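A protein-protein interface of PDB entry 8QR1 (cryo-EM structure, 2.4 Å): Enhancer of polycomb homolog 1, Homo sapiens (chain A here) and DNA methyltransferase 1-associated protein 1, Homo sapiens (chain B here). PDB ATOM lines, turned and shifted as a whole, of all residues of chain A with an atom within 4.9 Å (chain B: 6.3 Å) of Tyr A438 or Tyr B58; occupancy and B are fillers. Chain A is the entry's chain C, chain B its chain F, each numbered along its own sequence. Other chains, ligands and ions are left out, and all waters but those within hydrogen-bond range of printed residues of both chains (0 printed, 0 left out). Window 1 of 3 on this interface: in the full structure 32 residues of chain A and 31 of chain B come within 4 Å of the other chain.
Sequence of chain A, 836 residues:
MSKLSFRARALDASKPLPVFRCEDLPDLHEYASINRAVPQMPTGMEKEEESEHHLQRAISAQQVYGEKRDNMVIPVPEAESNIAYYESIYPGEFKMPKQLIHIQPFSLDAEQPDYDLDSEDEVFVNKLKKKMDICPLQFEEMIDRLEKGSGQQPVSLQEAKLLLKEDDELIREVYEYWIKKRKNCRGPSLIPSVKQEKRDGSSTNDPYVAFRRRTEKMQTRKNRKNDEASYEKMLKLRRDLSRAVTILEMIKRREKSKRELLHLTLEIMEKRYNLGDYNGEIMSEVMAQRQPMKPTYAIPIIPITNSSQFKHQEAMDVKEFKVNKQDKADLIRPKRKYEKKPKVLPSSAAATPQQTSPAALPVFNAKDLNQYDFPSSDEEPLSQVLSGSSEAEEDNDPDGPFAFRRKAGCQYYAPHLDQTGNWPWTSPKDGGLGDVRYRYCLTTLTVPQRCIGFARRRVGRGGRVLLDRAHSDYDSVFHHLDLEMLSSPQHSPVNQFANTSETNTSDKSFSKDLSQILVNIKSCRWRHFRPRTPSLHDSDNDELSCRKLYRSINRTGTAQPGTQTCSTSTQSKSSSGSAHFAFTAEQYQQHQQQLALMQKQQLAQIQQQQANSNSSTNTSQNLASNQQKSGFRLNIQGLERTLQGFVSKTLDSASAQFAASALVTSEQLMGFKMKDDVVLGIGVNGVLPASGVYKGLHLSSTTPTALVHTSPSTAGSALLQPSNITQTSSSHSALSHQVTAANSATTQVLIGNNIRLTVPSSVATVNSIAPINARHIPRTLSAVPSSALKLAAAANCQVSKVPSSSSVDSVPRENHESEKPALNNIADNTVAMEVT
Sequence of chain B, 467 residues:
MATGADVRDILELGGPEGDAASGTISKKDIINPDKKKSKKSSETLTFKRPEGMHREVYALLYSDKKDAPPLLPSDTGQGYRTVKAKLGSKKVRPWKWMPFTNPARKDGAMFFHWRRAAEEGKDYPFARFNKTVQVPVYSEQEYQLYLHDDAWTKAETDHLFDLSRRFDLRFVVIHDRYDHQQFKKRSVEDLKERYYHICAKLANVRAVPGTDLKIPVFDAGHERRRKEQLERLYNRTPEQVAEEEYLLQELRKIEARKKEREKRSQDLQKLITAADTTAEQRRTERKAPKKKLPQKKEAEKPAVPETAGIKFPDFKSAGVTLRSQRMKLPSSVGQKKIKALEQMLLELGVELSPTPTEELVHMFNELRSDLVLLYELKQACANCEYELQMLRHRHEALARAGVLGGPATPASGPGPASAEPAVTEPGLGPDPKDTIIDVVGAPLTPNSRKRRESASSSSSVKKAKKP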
ATOM      1  N   PRO A 424     -29.188  15.128   9.966  1.00  0.00           N
ATOM      2  CA  PRO A 424     -28.356  16.187   9.374  1.00  0.00           C
ATOM      3  C   PRO A 424     -28.362  16.213   7.851  1.00  0.00           C
ATOM      4  O   PRO A 424     -27.869  17.191   7.275  1.00  0.00           O
ATOM      5  CB  PRO A 424     -26.954  15.878   9.909  1.00  0.00           C
ATOM      6  CG  PRO A 424     -27.165  15.045  11.087  1.00  0.00           C
ATOM      7  CD  PRO A 424     -28.378  14.238  10.815  1.00  0.00           C
ATOM      8  N   TRP A 425     -28.903  15.188   7.193  1.00  0.00           N
ATOM      9  CA  TRP A 425     -28.816  15.012   5.750  1.00  0.00           C
ATOM     10  C   TRP A 425     -30.186  14.614   5.227  1.00  0.00           C
ATOM     11  O   TRP A 425     -31.042  14.132   5.974  1.00  0.00           O
ATOM     12  CB  TRP A 425     -27.776  13.956   5.380  1.00  0.00           C
ATOM     13  CG  TRP A 425     -27.576  12.935   6.442  1.00  0.00           C
ATOM     14  CD1 TRP A 425     -26.530  12.847   7.308  1.00  0.00           C
ATOM     15  CD2 TRP A 425     -28.459  11.863   6.768  1.00  0.00           C
ATOM     16  NE1 TRP A 425     -26.703  11.778   8.151  1.00  0.00           N
ATOM     17  CE2 TRP A 425     -27.881  11.157   7.839  1.00  0.00           C
ATOM     18  CE3 TRP A 425     -29.680  11.426   6.255  1.00  0.00           C
ATOM     19  CZ2 TRP A 425     -28.480  10.044   8.404  1.00  0.00           C
ATOM     20  CZ3 TRP A 425     -30.274  10.322   6.817  1.00  0.00           C
ATOM     21  CH2 TRP A 425     -29.675   9.641   7.881  1.00  0.00           C
ATOM     22  N   THR A 426     -30.402  14.848   3.933  1.00  0.00           N
ATOM     23  CA  THR A 426     -31.722  14.791   3.309  1.00  0.00           C
ATOM     24  C   THR A 426     -32.703  15.749   3.976  1.00  0.00           C
ATOM     25  O   THR A 426     -33.917  15.512   3.938  1.00  0.00           O
ATOM     26  CB  THR A 426     -32.316  13.368   3.318  1.00  0.00           C
ATOM     27  OG1 THR A 426     -32.632  12.977   4.661  1.00  0.00           O
ATOM     28  CG2 THR A 426     -31.370  12.341   2.697  1.00  0.00           C
ATOM     29  N   SER A 427     -32.201  16.831   4.578  1.00  0.00           N
ATOM     30  CA  SER A 427     -32.945  17.592   5.579  1.00  0.00           C
ATOM     31  C   SER A 427     -32.405  19.018   5.596  1.00  0.00           C
ATOM     32  O   SER A 427     -31.368  19.285   6.223  1.00  0.00           O
ATOM     33  CB  SER A 427     -32.808  16.948   6.953  1.00  0.00           C
ATOM     34  OG  SER A 427     -33.222  15.597   6.928  1.00  0.00           O
ATOM     35  N   PRO A 428     -33.061  19.960   4.919  1.00  0.00           N
ATOM     36  CA  PRO A 428     -32.709  21.370   5.112  1.00  0.00           C
ATOM     37  C   PRO A 428     -33.152  21.863   6.482  1.00  0.00           C
ATOM     38  O   PRO A 428     -33.678  21.117   7.309  1.00  0.00           O
ATOM     39  CB  PRO A 428     -33.449  22.084   3.973  1.00  0.00           C
ATOM     40  CG  PRO A 428     -34.519  21.177   3.582  1.00  0.00           C
ATOM     41  CD  PRO A 428     -33.992  19.802   3.784  1.00  0.00           C
ATOM     42  N   GLY A 434     -29.095  21.422   8.742  1.00  0.00           N
ATOM     43  CA  GLY A 434     -28.502  21.575   7.428  1.00  0.00           C
ATOM     44  C   GLY A 434     -26.992  21.641   7.450  1.00  0.00           C
ATOM     45  O   GLY A 434     -26.419  22.709   7.217  1.00  0.00           O
ATOM     46  N   ASP A 435     -26.336  20.524   7.742  1.00  0.00           N
ATOM     47  CA  ASP A 435     -24.885  20.474   7.650  1.00  0.00           C
ATOM     48  C   ASP A 435     -24.482  20.673   6.195  1.00  0.00           C
ATOM     49  O   ASP A 435     -24.893  19.908   5.317  1.00  0.00           O
ATOM     50  CB  ASP A 435     -24.366  19.149   8.197  1.00  0.00           C
ATOM     51  CG  ASP A 435     -22.855  19.116   8.329  1.00  0.00           C
ATOM     52  OD1 ASP A 435     -22.191  20.128   8.024  1.00  0.00           O
ATOM     53  OD2 ASP A 435     -22.329  18.067   8.753  1.00  0.00           O
ATOM     54  N   VAL A 436     -23.678  21.707   5.945  1.00  0.00           N
ATOM     55  CA  VAL A 436     -23.471  22.200   4.588  1.00  0.00           C
ATOM     56  C   VAL A 436     -22.677  21.237   3.718  1.00  0.00           C
ATOM     57  O   VAL A 436     -22.663  21.394   2.493  1.00  0.00           O
ATOM     58  CB  VAL A 436     -22.789  23.587   4.621  1.00  0.00           C
ATOM     59  CG1 VAL A 436     -23.652  24.578   5.375  1.00  0.00           C
ATOM     60  CG2 VAL A 436     -21.373  23.525   5.206  1.00  0.00           C
ATOM     61  N   ARG A 437     -22.006  20.246   4.308  1.00  0.00           N
ATOM     62  CA  ARG A 437     -21.256  19.299   3.489  1.00  0.00           C
ATOM     63  C   ARG A 437     -22.190  18.433   2.651  1.00  0.00           C
ATOM     64  O   ARG A 437     -21.788  17.944   1.587  1.00  0.00           O
ATOM     65  CB  ARG A 437     -20.319  18.462   4.377  1.00  0.00           C
ATOM     66  CG  ARG A 437     -20.753  17.046   4.780  1.00  0.00           C
ATOM     67  CD  ARG A 437     -19.673  16.366   5.607  1.00  0.00           C
ATOM     68  NE  ARG A 437     -19.483  16.967   6.926  1.00  0.00           N
ATOM     69  CZ  ARG A 437     -19.880  16.461   8.089  1.00  0.00           C
ATOM     70  NH1 ARG A 437     -20.582  15.341   8.173  1.00  0.00           N
ATOM     71  NH2 ARG A 437     -19.571  17.108   9.209  1.00  0.00           N
ATOM     72  N   TYR A 438     -23.427  18.232   3.103  1.00  0.00           N
ATOM     73  CA  TYR A 438     -24.452  17.540   2.334  1.00  0.00           C
ATOM     74  C   TYR A 438     -25.268  18.465   1.438  1.00  0.00           C
ATOM     75  O   TYR A 438     -26.180  17.985   0.757  1.00  0.00           O
ATOM     76  CB  TYR A 438     -25.406  16.809   3.276  1.00  0.00           C
ATOM     77  CG  TYR A 438     -24.720  15.997   4.341  1.00  0.00           C
ATOM     78  CD1 TYR A 438     -23.989  14.867   4.023  1.00  0.00           C
ATOM     79  CD2 TYR A 438     -24.813  16.357   5.671  1.00  0.00           C
ATOM     80  CE1 TYR A 438     -23.366  14.128   5.002  1.00  0.00           C
ATOM     81  CE2 TYR A 438     -24.194  15.626   6.652  1.00  0.00           C
ATOM     82  CZ  TYR A 438     -23.472  14.512   6.313  1.00  0.00           C
ATOM     83  OH  TYR A 438     -22.854  13.780   7.296  1.00  0.00           O
ATOM     84  N   ARG A 439     -24.971  19.762   1.419  1.00  0.00           N
ATOM     85  CA  ARG A 439     -25.763  20.720   0.663  1.00  0.00           C
ATOM     86  C   ARG A 439     -25.278  20.803  -0.774  1.00  0.00           C
ATOM     87  O   ARG A 439     -24.077  20.921  -1.033  1.00  0.00           O
ATOM     88  CB  ARG A 439     -25.682  22.098   1.317  1.00  0.00           C
ATOM     89  CG  ARG A 439     -26.616  23.151   0.729  1.00  0.00           C
ATOM     90  CD  ARG A 439     -26.419  24.499   1.384  1.00  0.00           C
ATOM     91  NE  ARG A 439     -25.096  25.054   1.122  1.00  0.00           N
ATOM     92  CZ  ARG A 439     -24.529  26.042   1.803  1.00  0.00           C
ATOM     93  NH1 ARG A 439     -25.158  26.664   2.788  1.00  0.00           N
ATOM     94  NH2 ARG A 439     -23.297  26.421   1.485  1.00  0.00           N
ATOM     95  N   TYR A 440     -26.227  20.758  -1.704  1.00  0.00           N
ATOM     96  CA  TYR A 440     -25.973  21.015  -3.114  1.00  0.00           C
ATOM     97  C   TYR A 440     -26.319  22.468  -3.403  1.00  0.00           C
ATOM     98  O   TYR A 440     -27.316  22.985  -2.890  1.00  0.00           O
ATOM     99  CB  TYR A 440     -26.802  20.112  -4.028  1.00  0.00           C
ATOM    100  CG  TYR A 440     -26.609  18.616  -3.911  1.00  0.00           C
ATOM    101  CD1 TYR A 440     -27.029  17.912  -2.795  1.00  0.00           C
ATOM    102  CD2 TYR A 440     -26.039  17.904  -4.948  1.00  0.00           C
ATOM    103  CE1 TYR A 440     -26.862  16.553  -2.710  1.00  0.00           C
ATOM    104  CE2 TYR A 440     -25.869  16.546  -4.870  1.00  0.00           C
ATOM    105  CZ  TYR A 440     -26.281  15.875  -3.750  1.00  0.00           C
ATOM    106  OH  TYR A 440     -26.110  14.517  -3.677  1.00  0.00           O
ATOM    107  N   ARG A 456     -22.527  19.427  -5.076  1.00  0.00           N
ATOM    108  CA  ARG A 456     -21.588  19.439  -3.963  1.00  0.00           C
ATOM    109  C   ARG A 456     -20.197  19.141  -4.488  1.00  0.00           C
ATOM    110  O   ARG A 456     -20.035  18.667  -5.612  1.00  0.00           O
ATOM    111  CB  ARG A 456     -21.881  18.384  -2.896  1.00  0.00           C
ATOM    112  CG  ARG A 456     -23.306  18.052  -2.655  1.00  0.00           C
ATOM    113  CD  ARG A 456     -23.451  17.048  -1.528  1.00  0.00           C
ATOM    114  NE  ARG A 456     -22.992  15.724  -1.936  1.00  0.00           N
ATOM    115  CZ  ARG A 456     -23.477  14.562  -1.513  1.00  0.00           C
ATOM    116  NH1 ARG A 456     -24.422  14.484  -0.591  1.00  0.00           N
ATOM    117  NH2 ARG A 456     -22.994  13.437  -2.029  1.00  0.00           N
ATOM    118  N   GLU B  56     -32.355  25.382  -2.246  1.00  0.00           N
ATOM    119  CA  GLU B  56     -31.214  24.493  -2.091  1.00  0.00           C
ATOM    120  C   GLU B  56     -31.742  23.147  -1.620  1.00  0.00           C
ATOM    121  O   GLU B  56     -32.828  23.060  -1.040  1.00  0.00           O
ATOM    122  CB  GLU B  56     -30.182  25.051  -1.103  1.00  0.00           C
ATOM    123  CG  GLU B  56     -30.739  25.427   0.272  1.00  0.00           C
ATOM    124  CD  GLU B  56     -29.737  26.178   1.125  1.00  0.00           C
ATOM    125  OE1 GLU B  56     -29.108  27.127   0.611  1.00  0.00           O
ATOM    126  OE2 GLU B  56     -29.583  25.824   2.313  1.00  0.00           O
ATOM    127  N   VAL B  57     -30.958  22.098  -1.878  1.00  0.00           N
ATOM    128  CA  VAL B  57     -31.343  20.723  -1.578  1.00  0.00           C
ATOM    129  C   VAL B  57     -30.211  20.031  -0.836  1.00  0.00           C
ATOM    130  O   VAL B  57     -29.035  20.374  -0.989  1.00  0.00           O
ATOM    131  CB  VAL B  57     -31.724  19.934  -2.854  1.00  0.00           C
ATOM    132  CG1 VAL B  57     -32.856  20.627  -3.582  1.00  0.00           C
ATOM    133  CG2 VAL B  57     -30.542  19.754  -3.779  1.00  0.00           C
ATOM    134  N   TYR B  58     -30.586  19.036  -0.030  1.00  0.00           N
ATOM    135  CA  TYR B  58     -29.682  18.271   0.814  1.00  0.00           C
ATOM    136  C   TYR B  58     -29.926  16.790   0.580  1.00  0.00           C
ATOM    137  O   TYR B  58     -31.054  16.380   0.294  1.00  0.00           O
ATOM    138  CB  TYR B  58     -29.894  18.575   2.300  1.00  0.00           C
ATOM    139  CG  TYR B  58     -29.538  19.971   2.757  1.00  0.00           C
ATOM    140  CD1 TYR B  58     -30.310  21.062   2.402  1.00  0.00           C
ATOM    141  CD2 TYR B  58     -28.446  20.190   3.579  1.00  0.00           C
ATOM    142  CE1 TYR B  58     -29.993  22.328   2.827  1.00  0.00           C
ATOM    143  CE2 TYR B  58     -28.124  21.453   4.012  1.00  0.00           C
ATOM    144  CZ  TYR B  58     -28.901  22.519   3.634  1.00  0.00           C
ATOM    145  OH  TYR B  58     -28.585  23.785   4.062  1.00  0.00           O
ATOM    146  N   ALA B  59     -28.871  15.990   0.708  1.00  0.00           N
ATOM    147  CA  ALA B  59     -28.994  14.547   0.572  1.00  0.00           C
ATOM    148  C   ALA B  59     -27.710  13.889   1.044  1.00  0.00           C
ATOM    149  O   ALA B  59     -26.627  14.476   0.972  1.00  0.00           O
ATOM    150  CB  ALA B  59     -29.299  14.137  -0.868  1.00  0.00           C
ATOM    151  N   LEU B  60     -27.847  12.656   1.532  1.00  0.00           N
ATOM    152  CA  LEU B  60     -26.699  11.884   1.986  1.00  0.00           C
ATOM    153  C   LEU B  60     -26.015  11.191   0.815  1.00  0.00           C
ATOM    154  O   LEU B  60     -24.890  11.546   0.457  1.00  0.00           O
ATOM    155  CB  LEU B  60     -27.139  10.861   3.035  1.00  0.00           C
ATOM    156  CG  LEU B  60     -26.084   9.950   3.663  1.00  0.00           C
ATOM    157  CD1 LEU B  60     -25.002  10.748   4.347  1.00  0.00           C
ATOM    158  CD2 LEU B  60     -26.742   9.014   4.641  1.00  0.00           C
ATOM    159  N   TYR B  62     -27.767  10.476  -2.528  1.00  0.00           N
ATOM    160  CA  TYR B  62     -28.208  11.243  -3.679  1.00  0.00           C
ATOM    161  C   TYR B  62     -29.642  11.685  -3.436  1.00  0.00           C
ATOM    162  O   TYR B  62     -30.366  11.092  -2.632  1.00  0.00           O
ATOM    163  CB  TYR B  62     -28.081  10.438  -4.978  1.00  0.00           C
ATOM    164  CG  TYR B  62     -28.680   9.052  -4.933  1.00  0.00           C
ATOM    165  CD1 TYR B  62     -30.029   8.845  -5.174  1.00  0.00           C
ATOM    166  CD2 TYR B  62     -27.889   7.947  -4.662  1.00  0.00           C
ATOM    167  CE1 TYR B  62     -30.574   7.583  -5.136  1.00  0.00           C
ATOM    168  CE2 TYR B  62     -28.424   6.681  -4.622  1.00  0.00           C
ATOM    169  CZ  TYR B  62     -29.768   6.504  -4.860  1.00  0.00           C
ATOM    170  OH  TYR B  62     -30.308   5.242  -4.823  1.00  0.00           O
ATOM    171  N   SER B  63     -30.041  12.742  -4.142  1.00  0.00           N
ATOM    172  CA  SER B  63     -31.352  13.335  -3.919  1.00  0.00           C
ATOM    173  C   SER B  63     -32.471  12.496  -4.522  1.00  0.00           C
ATOM    174  O   SER B  63     -33.541  12.364  -3.919  1.00  0.00           O
ATOM    175  CB  SER B  63     -31.387  14.747  -4.499  1.00  0.00           C
ATOM    176  OG  SER B  63     -30.463  15.588  -3.837  1.00  0.00           O
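O of Leu B60 is in hydrogen-bond range of NH1 of Arg A456, 3.2 Å away.
N of Tyr A440 is in hydrogen-bond range of O of Val B57 (2.9 Å).
The guanidinium group of Arg A456 sits at hydrogen-bond distance from the backbone carbonyl oxygen of Ala B59, 2.7 Å away.
The backbone carbonyl oxygen of Tyr A438 lies within hydrogen-bond range of the backbone NH of Ala B59, 3.4 Å away.
The side-chain hydroxyl of Ser A427 lies within hydrogen-bond range of the backbone carbonyl oxygen of Trp A425.
OH of Tyr A438 lies within hydrogen-bond range of NH1 of Arg A437, 2.9 Å away.
The side-chain carboxylate of Asp A435 is in salt-bridge range of the guanidinium group of Arg A437 (3.0 Å).
The side-chain carboxylate (OE2) of Glu B56 is in hydrogen-bond range of the side-chain hydroxyl (OH) of Tyr B58, 2.9 Å away.
Among the printed residues, pairs that only touch across the chains: Gly A434 with Tyr B58 (3.4 Å), Thr A426 with Tyr B58 (3.5 Å), Tyr A438 with Tyr B58 (3.5 Å), Arg A439 with Tyr B58 (3.5 Å), Arg A439 with Glu B56 (3.6 Å), Pro A428 with Tyr B58 (3.6 Å), Thr A426 with Ala B59 (3.7 Å), Ser A427 with Tyr B58 (3.7 Å), Arg A439 with Val B57 (3.7 Å), Thr A426 with Leu B60 (3.7 Å), Asp A435 with Tyr B58 (3.8 Å), Tyr A438 with Leu B60 (3.8 Å), Tyr A440 with Tyr B62 (3.9 Å), Tyr A440 with Ser B63 (3.9 Å), Tyr A440 with Ala B59 (3.9 Å), Trp A425 with Leu B60 (3.9 Å) and Tyr A440 with Glu B56 (3.96 Å).
Printed residues of chain B within 4 Å of Tyr A438: Tyr B58, Ala B59 and Leu B60.
Of the printed residues of chain A, Tyr B58 touches Thr A426, Ser A427, Pro A428, Gly A434, Asp A435, Tyr A438 and Arg A439.
Printed residues of chain B within 4 Å of Gly A434: Tyr B58 (3.4 Å).
Of the printed residues of chain B, Ser A427 touches Tyr B58.
Pro A424 touches none of the printed residues of chain B.
The nearest residue of chain B that does not touch Tyr A438 is Val B57 (4.1 Å).
The nearest residue of chain A that does not touch Tyr B58 is Tyr A440 (4.5 Å).
The nearest printed residue of chain A that does not touch Leu B60 is Tyr A440 (5.2 Å).
Hydrophobic or aromatic side chains of chain A that line the printed part of chain B: Trp A425, Pro A428, Tyr A438 and Tyr A440.
Along chain A the printed residues that touch a printed residue of chain B span positions 425 to 456.
Printed residues of chain B that touch a printed residue of chain A: Glu B56, Val B57, Tyr B58, Ala B59, Leu B60, Tyr B62 and Ser B63.
Among the printed residues, 21 pairs touch across the chains.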
